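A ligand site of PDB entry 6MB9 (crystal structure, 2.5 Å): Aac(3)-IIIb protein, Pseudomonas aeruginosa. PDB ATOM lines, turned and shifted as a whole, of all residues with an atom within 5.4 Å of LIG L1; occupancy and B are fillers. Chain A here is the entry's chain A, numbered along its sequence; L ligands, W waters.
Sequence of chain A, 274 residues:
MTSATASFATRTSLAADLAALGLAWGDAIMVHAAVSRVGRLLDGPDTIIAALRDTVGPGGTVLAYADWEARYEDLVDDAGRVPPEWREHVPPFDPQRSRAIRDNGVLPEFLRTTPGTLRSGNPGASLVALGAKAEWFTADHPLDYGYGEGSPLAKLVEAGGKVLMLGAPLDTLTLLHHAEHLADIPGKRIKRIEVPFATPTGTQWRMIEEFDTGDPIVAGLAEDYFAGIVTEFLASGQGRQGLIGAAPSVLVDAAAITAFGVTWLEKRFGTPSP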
ATOM      1  N   TYR A  65       4.179  21.215 -17.536  1.00  0.00           N
ATOM      2  CA  TYR A  65       5.319  21.348 -16.643  1.00  0.00           C
ATOM      3  C   TYR A  65       4.883  21.002 -15.228  1.00  0.00           C
ATOM      4  O   TYR A  65       4.027  21.690 -14.647  1.00  0.00           O
ATOM      5  CB  TYR A  65       5.909  22.754 -16.705  1.00  0.00           C
ATOM      6  CG  TYR A  65       7.110  22.975 -15.821  1.00  0.00           C
ATOM      7  CD1 TYR A  65       8.134  22.039 -15.757  1.00  0.00           C
ATOM      8  CD2 TYR A  65       7.251  24.140 -15.079  1.00  0.00           C
ATOM      9  CE1 TYR A  65       9.246  22.237 -14.953  1.00  0.00           C
ATOM     10  CE2 TYR A  65       8.347  24.352 -14.266  1.00  0.00           C
ATOM     11  CZ  TYR A  65       9.345  23.399 -14.215  1.00  0.00           C
ATOM     12  OH  TYR A  65      10.448  23.618 -13.412  1.00  0.00           O
ATOM     13  N   ASP A  67       7.128  20.168 -12.334  1.00  0.00           N
ATOM     14  CA  ASP A  67       8.004  20.638 -11.259  1.00  0.00           C
ATOM     15  C   ASP A  67       7.814  19.707 -10.066  1.00  0.00           C
ATOM     16  O   ASP A  67       7.414  18.540 -10.227  1.00  0.00           O
ATOM     17  CB  ASP A  67       7.748  22.117 -10.974  1.00  0.00           C
ATOM     18  CG  ASP A  67       8.935  22.814 -10.292  1.00  0.00           C
ATOM     19  OD1 ASP A  67       9.717  22.124  -9.606  1.00  0.00           O
ATOM     20  OD2 ASP A  67       9.089  24.035 -10.457  1.00  0.00           O
ATOM     21  N   GLU A  73      13.365  23.413   0.379  1.00  0.00           N
ATOM     22  CA  GLU A  73      14.369  24.314  -0.155  1.00  0.00           C
ATOM     23  C   GLU A  73      14.679  25.472   0.772  1.00  0.00           C
ATOM     24  O   GLU A  73      15.797  26.014   0.751  1.00  0.00           O
ATOM     25  CB  GLU A  73      13.944  24.866  -1.517  1.00  0.00           C
ATOM     26  CG  GLU A  73      14.381  23.961  -2.621  1.00  0.00           C
ATOM     27  CD  GLU A  73      14.622  24.683  -3.928  1.00  0.00           C
ATOM     28  OE1 GLU A  73      14.205  25.850  -4.065  1.00  0.00           O
ATOM     29  OE2 GLU A  73      15.257  24.071  -4.810  1.00  0.00           O
ATOM     30  N   ASP A 103       2.399  26.153  -7.822  1.00  0.00           N
ATOM     31  CA  ASP A 103       2.509  27.405  -8.567  1.00  0.00           C
ATOM     32  C   ASP A 103       2.089  27.227 -10.024  1.00  0.00           C
ATOM     33  O   ASP A 103       1.570  28.175 -10.634  1.00  0.00           O
ATOM     34  CB  ASP A 103       3.936  27.934  -8.497  1.00  0.00           C
ATOM     35  CG  ASP A 103       4.488  27.946  -7.076  1.00  0.00           C
ATOM     36  OD1 ASP A 103       5.713  28.130  -6.920  1.00  0.00           O
ATOM     37  OD2 ASP A 103       3.700  27.748  -6.127  1.00  0.00           O
ATOM     38  N   GLY A 124      12.802  18.925 -10.268  1.00  0.00           N
ATOM     39  CA  GLY A 124      12.534  20.332 -10.490  1.00  0.00           C
ATOM     40  C   GLY A 124      12.177  20.661 -11.921  1.00  0.00           C
ATOM     41  O   GLY A 124      11.442  21.623 -12.169  1.00  0.00           O
ATOM     42  N   TYR A 147      17.173  21.166 -18.106  1.00  0.00           N
ATOM     43  CA  TYR A 147      16.508  22.003 -19.104  1.00  0.00           C
ATOM     44  C   TYR A 147      17.293  22.059 -20.403  1.00  0.00           C
ATOM     45  O   TYR A 147      17.026  22.933 -21.240  1.00  0.00           O
ATOM     46  CB  TYR A 147      16.274  23.415 -18.556  1.00  0.00           C
ATOM     47  CG  TYR A 147      15.486  23.444 -17.266  1.00  0.00           C
ATOM     48  CD1 TYR A 147      14.115  23.649 -17.274  1.00  0.00           C
ATOM     49  CD2 TYR A 147      16.118  23.251 -16.039  1.00  0.00           C
ATOM     50  CE1 TYR A 147      13.391  23.675 -16.095  1.00  0.00           C
ATOM     51  CE2 TYR A 147      15.398  23.268 -14.865  1.00  0.00           C
ATOM     52  CZ  TYR A 147      14.038  23.472 -14.886  1.00  0.00           C
ATOM     53  OH  TYR A 147      13.336  23.497 -13.712  1.00  0.00           O
ATOM     54  N   ASP A 171       4.950  34.866 -19.406  1.00  0.00           N
ATOM     55  CA  ASP A 171       6.245  34.611 -18.782  1.00  0.00           C
ATOM     56  C   ASP A 171       6.362  33.222 -18.154  1.00  0.00           C
ATOM     57  O   ASP A 171       7.432  32.877 -17.656  1.00  0.00           O
ATOM     58  CB  ASP A 171       6.537  35.687 -17.720  1.00  0.00           C
ATOM     59  CG  ASP A 171       5.507  35.718 -16.615  1.00  0.00           C
ATOM     60  OD1 ASP A 171       5.650  34.941 -15.640  1.00  0.00           O
ATOM     61  OD2 ASP A 171       4.543  36.507 -16.716  1.00  0.00           O
ATOM     62  N   THR A 172       5.295  32.424 -18.168  1.00  0.00           N
ATOM     63  CA  THR A 172       5.315  31.084 -17.601  1.00  0.00           C
ATOM     64  C   THR A 172       5.670  30.015 -18.625  1.00  0.00           C
ATOM     65  O   THR A 172       5.526  28.824 -18.340  1.00  0.00           O
ATOM     66  CB  THR A 172       3.959  30.756 -16.961  1.00  0.00           C
ATOM     67  OG1 THR A 172       2.957  30.673 -17.991  1.00  0.00           O
ATOM     68  CG2 THR A 172       3.568  31.833 -15.961  1.00  0.00           C
ATOM     69  N   HIS A 177      13.167  28.433 -20.735  1.00  0.00           N
ATOM     70  CA  HIS A 177      14.320  28.058 -19.926  1.00  0.00           C
ATOM     71  C   HIS A 177      15.273  27.176 -20.711  1.00  0.00           C
ATOM     72  O   HIS A 177      16.487  27.205 -20.462  1.00  0.00           O
ATOM     73  CB  HIS A 177      13.852  27.332 -18.656  1.00  0.00           C
ATOM     74  CG  HIS A 177      13.172  28.218 -17.668  1.00  0.00           C
ATOM     75  ND1 HIS A 177      13.744  29.376 -17.192  1.00  0.00           N
ATOM     76  CD2 HIS A 177      11.970  28.120 -17.063  1.00  0.00           C
ATOM     77  CE1 HIS A 177      12.916  29.956 -16.332  1.00  0.00           C
ATOM     78  NE2 HIS A 177      11.830  29.208 -16.245  1.00  0.00           N
ATOM     79  N   LYS A 191      22.410  27.206 -10.169  1.00  0.00           N
ATOM     80  CA  LYS A 191      21.747  26.690  -8.987  1.00  0.00           C
ATOM     81  C   LYS A 191      22.303  25.327  -8.614  1.00  0.00           C
ATOM     82  O   LYS A 191      22.403  24.439  -9.465  1.00  0.00           O
ATOM     83  CB  LYS A 191      20.237  26.595  -9.176  1.00  0.00           C
ATOM     84  CG  LYS A 191      19.561  26.034  -7.934  1.00  0.00           C
ATOM     85  CD  LYS A 191      18.072  25.834  -8.081  1.00  0.00           C
ATOM     86  CE  LYS A 191      17.488  25.314  -6.773  1.00  0.00           C
ATOM     87  NZ  LYS A 191      16.187  25.947  -6.405  1.00  0.00           N
ATOM     88  N   ASP A 212      20.110  28.494 -12.949  1.00  0.00           N
ATOM     89  CA  ASP A 212      19.028  28.855 -12.042  1.00  0.00           C
ATOM     90  C   ASP A 212      17.818  29.343 -12.839  1.00  0.00           C
ATOM     91  O   ASP A 212      17.920  30.295 -13.626  1.00  0.00           O
ATOM     92  CB  ASP A 212      19.512  29.933 -11.069  1.00  0.00           C
ATOM     93  CG  ASP A 212      18.499  30.237  -9.979  1.00  0.00           C
ATOM     94  OD1 ASP A 212      17.614  29.402  -9.735  1.00  0.00           O
ATOM     95  OD2 ASP A 212      18.622  31.310  -9.357  1.00  0.00           O
ATOM     96  N   THR A 213      16.682  28.667 -12.672  1.00  0.00           N
ATOM     97  CA  THR A 213      15.441  29.054 -13.329  1.00  0.00           C
ATOM     98  C   THR A 213      14.494  29.820 -12.417  1.00  0.00           C
ATOM     99  O   THR A 213      13.403  30.193 -12.867  1.00  0.00           O
ATOM    100  CB  THR A 213      14.725  27.821 -13.896  1.00  0.00           C
ATOM    101  OG1 THR A 213      14.414  26.916 -12.835  1.00  0.00           O
ATOM    102  CG2 THR A 213      15.593  27.107 -14.937  1.00  0.00           C
ATOM    103  N   GLY A 214      14.876  30.053 -11.161  1.00  0.00           N
ATOM    104  CA  GLY A 214      14.069  30.876 -10.273  1.00  0.00           C
ATOM    105  C   GLY A 214      14.156  32.364 -10.539  1.00  0.00           C
ATOM    106  O   GLY A 214      13.374  33.135  -9.970  1.00  0.00           O
ATOM    107  N   ASP A 215      15.092  32.783 -11.382  1.00  0.00           N
ATOM    108  CA  ASP A 215      15.242  34.164 -11.789  1.00  0.00           C
ATOM    109  C   ASP A 215      15.743  34.168 -13.221  1.00  0.00           C
ATOM    110  O   ASP A 215      16.112  33.112 -13.761  1.00  0.00           O
ATOM    111  CB  ASP A 215      16.202  34.921 -10.878  1.00  0.00           C
ATOM    112  CG  ASP A 215      15.486  35.866  -9.925  1.00  0.00           C
ATOM    113  OD1 ASP A 215      16.010  36.115  -8.830  1.00  0.00           O
ATOM    114  OD2 ASP A 215      14.382  36.327 -10.273  1.00  0.00           O
ATOM    115  N   GLU A 223      11.984  40.097 -14.091  1.00  0.00           N
ATOM    116  CA  GLU A 223      11.556  38.762 -13.692  1.00  0.00           C
ATOM    117  C   GLU A 223      10.667  38.113 -14.748  1.00  0.00           C
ATOM    118  O   GLU A 223      10.804  36.922 -15.049  1.00  0.00           O
ATOM    119  CB  GLU A 223      10.849  38.833 -12.346  1.00  0.00           C
ATOM    120  CG  GLU A 223      11.040  37.620 -11.454  1.00  0.00           C
ATOM    121  CD  GLU A 223      10.403  37.784 -10.095  1.00  0.00           C
ATOM    122  OE1 GLU A 223      10.896  38.622  -9.306  1.00  0.00           O
ATOM    123  OE2 GLU A 223       9.410  37.082  -9.800  1.00  0.00           O
ATOM    124  N   ASP A 224       9.727  38.875 -15.322  1.00  0.00           N
ATOM    125  CA  ASP A 224       8.793  38.366 -16.314  1.00  0.00           C
ATOM    126  C   ASP A 224       9.261  38.608 -17.755  1.00  0.00           C
ATOM    127  O   ASP A 224       8.423  38.740 -18.652  1.00  0.00           O
ATOM    128  CB  ASP A 224       7.406  38.989 -16.099  1.00  0.00           C
ATOM    129  CG  ASP A 224       7.445  40.503 -16.083  1.00  0.00           C
ATOM    130  OD1 ASP A 224       8.544  41.072 -15.905  1.00  0.00           O
ATOM    131  OD2 ASP A 224       6.376  41.123 -16.265  1.00  0.00           O
ATOM    132  N   PHE A 226      10.329  36.775 -19.996  1.00  0.00           N
ATOM    133  CA  PHE A 226       9.896  35.809 -20.988  1.00  0.00           C
ATOM    134  C   PHE A 226       8.712  36.337 -21.797  1.00  0.00           C
ATOM    135  O   PHE A 226       8.632  36.133 -23.009  1.00  0.00           O
ATOM    136  CB  PHE A 226       9.525  34.478 -20.325  1.00  0.00           C
ATOM    137  CG  PHE A 226      10.698  33.583 -20.043  1.00  0.00           C
ATOM    138  CD1 PHE A 226      11.986  33.956 -20.412  1.00  0.00           C
ATOM    139  CD2 PHE A 226      10.517  32.367 -19.412  1.00  0.00           C
ATOM    140  CE1 PHE A 226      13.054  33.132 -20.148  1.00  0.00           C
ATOM    141  CE2 PHE A 226      11.586  31.538 -19.161  1.00  0.00           C
ATOM    142  CZ  PHE A 226      12.858  31.925 -19.522  1.00  0.00           C
HETATM  143  C1  LIG L   1       9.138  31.480 -11.472  1.00  0.00           C
HETATM  144  O1  LIG L   1       8.878  30.129 -11.721  1.00  0.00           O
HETATM  145  C2  LIG L   1       7.913  32.093 -10.897  1.00  0.00           C
HETATM  146  N1  LIG L   1       7.397  31.164  -9.786  1.00  0.00           N
HETATM  147  C3  LIG L   1       6.839  32.269 -11.865  1.00  0.00           C
HETATM  148  O2  LIG L   1       5.740  33.002 -11.211  1.00  0.00           O
HETATM  149  C4  LIG L   1       7.276  33.020 -13.065  1.00  0.00           C
HETATM  150  O3  LIG L   1       6.213  33.038 -14.010  1.00  0.00           O
HETATM  151  C5  LIG L   1       8.508  32.384 -13.759  1.00  0.00           C
HETATM  152  O4  LIG L   1       9.602  32.163 -12.704  1.00  0.00           O
HETATM  153  C6  LIG L   1       8.970  33.267 -14.769  1.00  0.00           C
HETATM  154  C7  LIG L   1      11.131  26.627 -12.025  1.00  0.00           C
HETATM  155  N2  LIG L   1      12.194  25.634 -12.231  1.00  0.00           N
HETATM  156  C8  LIG L   1      11.560  27.608 -10.918  1.00  0.00           C
HETATM  157  C9  LIG L   1      10.493  28.665 -10.653  1.00  0.00           C
HETATM  158  O5  LIG L   1      11.016  29.645  -9.738  1.00  0.00           O
HETATM  159  C10 LIG L   1      10.056  29.381 -11.948  1.00  0.00           C
HETATM  160  C11 LIG L   1       9.743  28.407 -13.096  1.00  0.00           C
HETATM  161  N3  LIG L   1       9.493  29.169 -14.331  1.00  0.00           N
HETATM  162  C12 LIG L   1      10.851  27.383 -13.322  1.00  0.00           C
HETATM  163  C13 LIG L   1      10.642  29.404  -8.445  1.00  0.00           C
HETATM  164  C14 LIG L   1      11.713  29.493  -7.644  1.00  0.00           C
HETATM  165  C15 LIG L   1      11.700  30.967  -7.188  1.00  0.00           C
HETATM  166  C16 LIG L   1      10.149  31.227  -6.966  1.00  0.00           C
HETATM  167  O6  LIG L   1       9.580  30.565  -7.944  1.00  0.00           O
HETATM  168  C17 LIG L   1       9.798  32.710  -7.045  1.00  0.00           C
HETATM  169  C18 LIG L   1      14.721  34.606  -5.670  1.00  0.00           C
HETATM  170  C19 LIG L   1      15.331  33.295  -5.309  1.00  0.00           C
HETATM  171  C20 LIG L   1      14.342  32.209  -5.146  1.00  0.00           C
HETATM  172  C21 LIG L   1      13.466  32.076  -6.337  1.00  0.00           C
HETATM  173  O7  LIG L   1      12.420  31.134  -6.052  1.00  0.00           O
HETATM  174  C22 LIG L   1      13.852  34.505  -6.949  1.00  0.00           C
HETATM  175  O8  LIG L   1      12.840  33.346  -6.723  1.00  0.00           O
HETATM  176  C23 LIG L   1      13.151  35.701  -7.166  1.00  0.00           C
HETATM  177  N4  LIG L   1       9.746  32.542 -15.765  1.00  0.00           N
HETATM  178  O9  LIG L   1      11.573  28.596  -6.480  1.00  0.00           O
HETATM  179  O10 LIG L   1      16.265  32.921  -6.369  1.00  0.00           O
HETATM  180  O11 LIG L   1      13.886  35.031  -4.586  1.00  0.00           O
HETATM  181  O12 LIG L   1       9.580  33.101  -8.389  1.00  0.00           O
HETATM  182  O13 LIG L   1      11.805  26.854  -9.755  1.00  0.00           O
HETATM  183  N5  LIG L   1      12.001  35.434  -8.056  1.00  0.00           N
HETATM  184  N6  LIG L   1      13.461  32.462  -3.936  1.00  0.00           N
HETATM  185  N1  LG2 L   2     -11.603  20.902  -8.671  1.00  0.00           N
HETATM  186  C1  LG2 L   2     -12.264  21.462  -9.725  1.00  0.00           C
HETATM  187  N2  LG2 L   2     -11.828  22.642 -10.263  1.00  0.00           N
HETATM  188  C2  LG2 L   2     -10.731  23.258  -9.760  1.00  0.00           C
HETATM  189  C3  LG2 L   2     -10.079  22.718  -8.729  1.00  0.00           C
HETATM  190  C4  LG2 L   2     -10.535  21.510  -8.176  1.00  0.00           C
HETATM  191  N3  LG2 L   2     -10.009  20.752  -7.089  1.00  0.00           N
HETATM  192  N4  LG2 L   2      -9.044  23.529  -8.420  1.00  0.00           N
HETATM  193  C5  LG2 L   2      -9.060  24.555  -9.265  1.00  0.00           C
HETATM  194  N5  LG2 L   2     -10.106  24.406 -10.094  1.00  0.00           N
HETATM  195  C6  LG2 L   2     -10.531  25.260 -11.173  1.00  0.00           C
HETATM  196  C7  LG2 L   2     -11.310  26.228 -10.746  1.00  0.00           C
HETATM  197  O1  LG2 L   2     -12.223  26.587 -11.790  1.00  0.00           O
HETATM  198  C8  LG2 L   2     -10.360  27.428 -10.486  1.00  0.00           C
HETATM  199  O2  LG2 L   2     -10.992  28.590 -10.673  1.00  0.00           O
HETATM  200  P1  LG2 L   2     -11.448  29.525  -9.325  1.00  0.00           P
HETATM  201  O3  LG2 L   2     -11.665  30.956  -9.754  1.00  0.00           O
HETATM  202  O4  LG2 L   2     -10.334  29.469  -8.251  1.00  0.00           O
HETATM  203  O5  LG2 L   2     -12.746  28.973  -8.784  1.00  0.00           O
HETATM  204  C9  LG2 L   2      -9.319  27.263 -11.646  1.00  0.00           C
HETATM  205  O6  LG2 L   2      -9.219  25.983 -11.866  1.00  0.00           O
HETATM  206  C10 LG2 L   2      -7.974  27.824 -11.242  1.00  0.00           C
HETATM  207  O7  LG2 L   2      -7.133  27.595 -12.337  1.00  0.00           O
HETATM  208  P2  LG2 L   2      -5.503  27.536 -12.068  1.00  0.00           P
HETATM  209  O8  LG2 L   2      -5.186  26.412 -11.131  1.00  0.00           O
HETATM  210  O9  LG2 L   2      -4.805  27.327 -13.379  1.00  0.00           O
HETATM  211  O10 LG2 L   2      -5.059  28.985 -11.420  1.00  0.00           O
HETATM  212  P3  LG2 L   2      -5.383  30.476 -12.167  1.00  0.00           P
HETATM  213  O11 LG2 L   2      -5.979  31.422 -11.137  1.00  0.00           O
HETATM  214  O12 LG2 L   2      -6.361  30.304 -13.312  1.00  0.00           O
HETATM  215  O13 LG2 L   2      -3.972  31.097 -12.733  1.00  0.00           O
HETATM  216  C11 LG2 L   2      -1.687  30.493 -12.471  1.00  0.00           C
HETATM  217  C12 LG2 L   2      -2.893  31.143 -11.809  1.00  0.00           C
HETATM  218  C13 LG2 L   2      -1.964  29.030 -12.598  1.00  0.00           C
HETATM  219  C14 LG2 L   2      -0.461  30.708 -11.605  1.00  0.00           C
HETATM  220  C15 LG2 L   2      -1.498  31.127 -13.858  1.00  0.00           C
HETATM  221  O14 LG2 L   2      -1.335  32.477 -13.690  1.00  0.00           O
HETATM  222  C16 LG2 L   2      -0.231  30.538 -14.551  1.00  0.00           C
HETATM  223  O15 LG2 L   2       0.853  31.089 -14.421  1.00  0.00           O
HETATM  224  N6  LG2 L   2      -0.348  29.284 -15.409  1.00  0.00           N
HETATM  225  C17 LG2 L   2       0.890  28.685 -16.079  1.00  0.00           C
HETATM  226  C18 LG2 L   2       1.512  27.746 -15.049  1.00  0.00           C
HETATM  227  C19 LG2 L   2       2.855  27.139 -15.512  1.00  0.00           C
HETATM  228  O16 LG2 L   2       2.893  26.270 -16.333  1.00  0.00           O
HETATM  229  N7  LG2 L   2       4.041  27.623 -14.902  1.00  0.00           N
HETATM  230  C20 LG2 L   2       5.360  27.104 -15.272  1.00  0.00           C
HETATM  231  C21 LG2 L   2       6.352  27.584 -14.170  1.00  0.00           C
HETATM  232  S1  LG2 L   2       6.226  29.424 -14.039  1.00  0.00           S
HETATM  233  O   HOH W   1       9.651  34.708 -11.473  1.00  0.00           O
HETATM  234  O   HOH W   2      11.963  23.757  -9.759  1.00  0.00           O
HETATM  235  O   HOH W   3       4.376  34.877  -8.887  1.00  0.00           O
HETATM  236  O   HOH W   4      13.127  33.270 -16.124  1.00  0.00           O
HETATM  237  O   HOH W   5       8.613  30.287 -17.164  1.00  0.00           O
HETATM  238  O   HOH W   6      10.191  25.215  -8.323  1.00  0.00           O
HETATM  239  O   HOH W   7       8.331  27.687 -16.475  1.00  0.00           O
HETATM  240  O   HOH W   8       9.558  26.861  -6.060  1.00  0.00           O
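Residues that only touch LIG L1: Thr 172 (3.5 Å) and Phe 226 (3.7 Å). Hydrophobic or aromatic side chains that line LIG L1: Tyr 147, His 177 and Phe 226. 11 residues have an atom within 4 Å of LIG L1: Tyr 65, Asp 67, Tyr 147, Asp 171, Thr 172, His 177, Thr 213, Gly 214, Asp 215, Glu 223 and Phe 226.
The backbone carbonyl oxygen (O) of Asp 171 sits at hydrogen-bond distance from a nitrogen (N4) of LIG L1 (3.0 Å). OD1 of Asp 171 lies within hydrogen-bond range of O3 of LIG L1. A nitrogen (N2) of LIG L1 sits at hydrogen-bond distance from the side-chain hydroxyl (OG1) of Thr 213, at 2.6 Å. OH of Tyr 147 sits at hydrogen-bond distance from N2 of LIG L1, 2.8 Å away. The side-chain hydroxyl (OH) of Tyr 65 lies within hydrogen-bond range of a nitrogen (N2) of LIG L1 (2.9 Å). A ring nitrogen (NE2) of His 177 is in hydrogen-bond range of a nitrogen (N3) of LIG L1, at 3.0 Å. The side-chain carboxylate (OD2) of Asp 215 is in salt-bridge range of a nitrogen (N5) of LIG L1 (3.4 Å). The backbone carbonyl oxygen (O) of Gly 214 is in hydrogen-bond range of a nitrogen (N5) of LIG L1, at 3.3 Å. OE2 of Glu 223 lies within salt-bridge range of N5 of LIG L1, 3.5 Å away. OD2 of Asp 67 lies within salt-bridge range of N2 of LIG L1 (3.9 Å).
A nitrogen (N3) of LIG L1 sits close to a sulfur (S1) of LG2 L2 (3.3 Å).
OH of Tyr 147 is in hydrogen-bond range of OH of Tyr 65, 2.9 Å away. The side-chain hydroxyl (OH) of Tyr 147 sits at hydrogen-bond distance from the backbone carbonyl oxygen (O) of Gly 124 (3.1 Å). The side-chain carboxylate (OD2) of Asp 67 is in hydrogen-bond range of the side-chain hydroxyl (OH) of Tyr 65 (3.3 Å). The backbone carbonyl oxygen (O) of Gly 124 lies within hydrogen-bond range of the side-chain hydroxyl (OH) of Tyr 65, 2.6 Å away. N of Gly 214 sits at hydrogen-bond distance from OD1 of Asp 212 (3.2 Å).
Water W6 bridges the side-chain carboxylate of Asp 67 (2.7 Å) and an oxygen (O13) of LIG L1 (2.7 Å). Water W1 lies within hydrogen-bond range of an oxygen (O4) of LIG L1 (2.8 Å) and the side-chain carboxylate (OE2) of Glu 223 (2.9 Å). Water W7 lies within hydrogen-bond range of N3 of LIG L1 (2.9 Å) and S1 of LG2 L2 (3.7 Å). Water W5 lies within hydrogen-bond range of N4 of LIG L1 and O of Asp 171. Water W2 lies within hydrogen-bond range of OD1 of Asp 67 (2.8 Å), O13 of LIG L1 (3.1 Å) and O of Gly 124 (3.3 Å).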
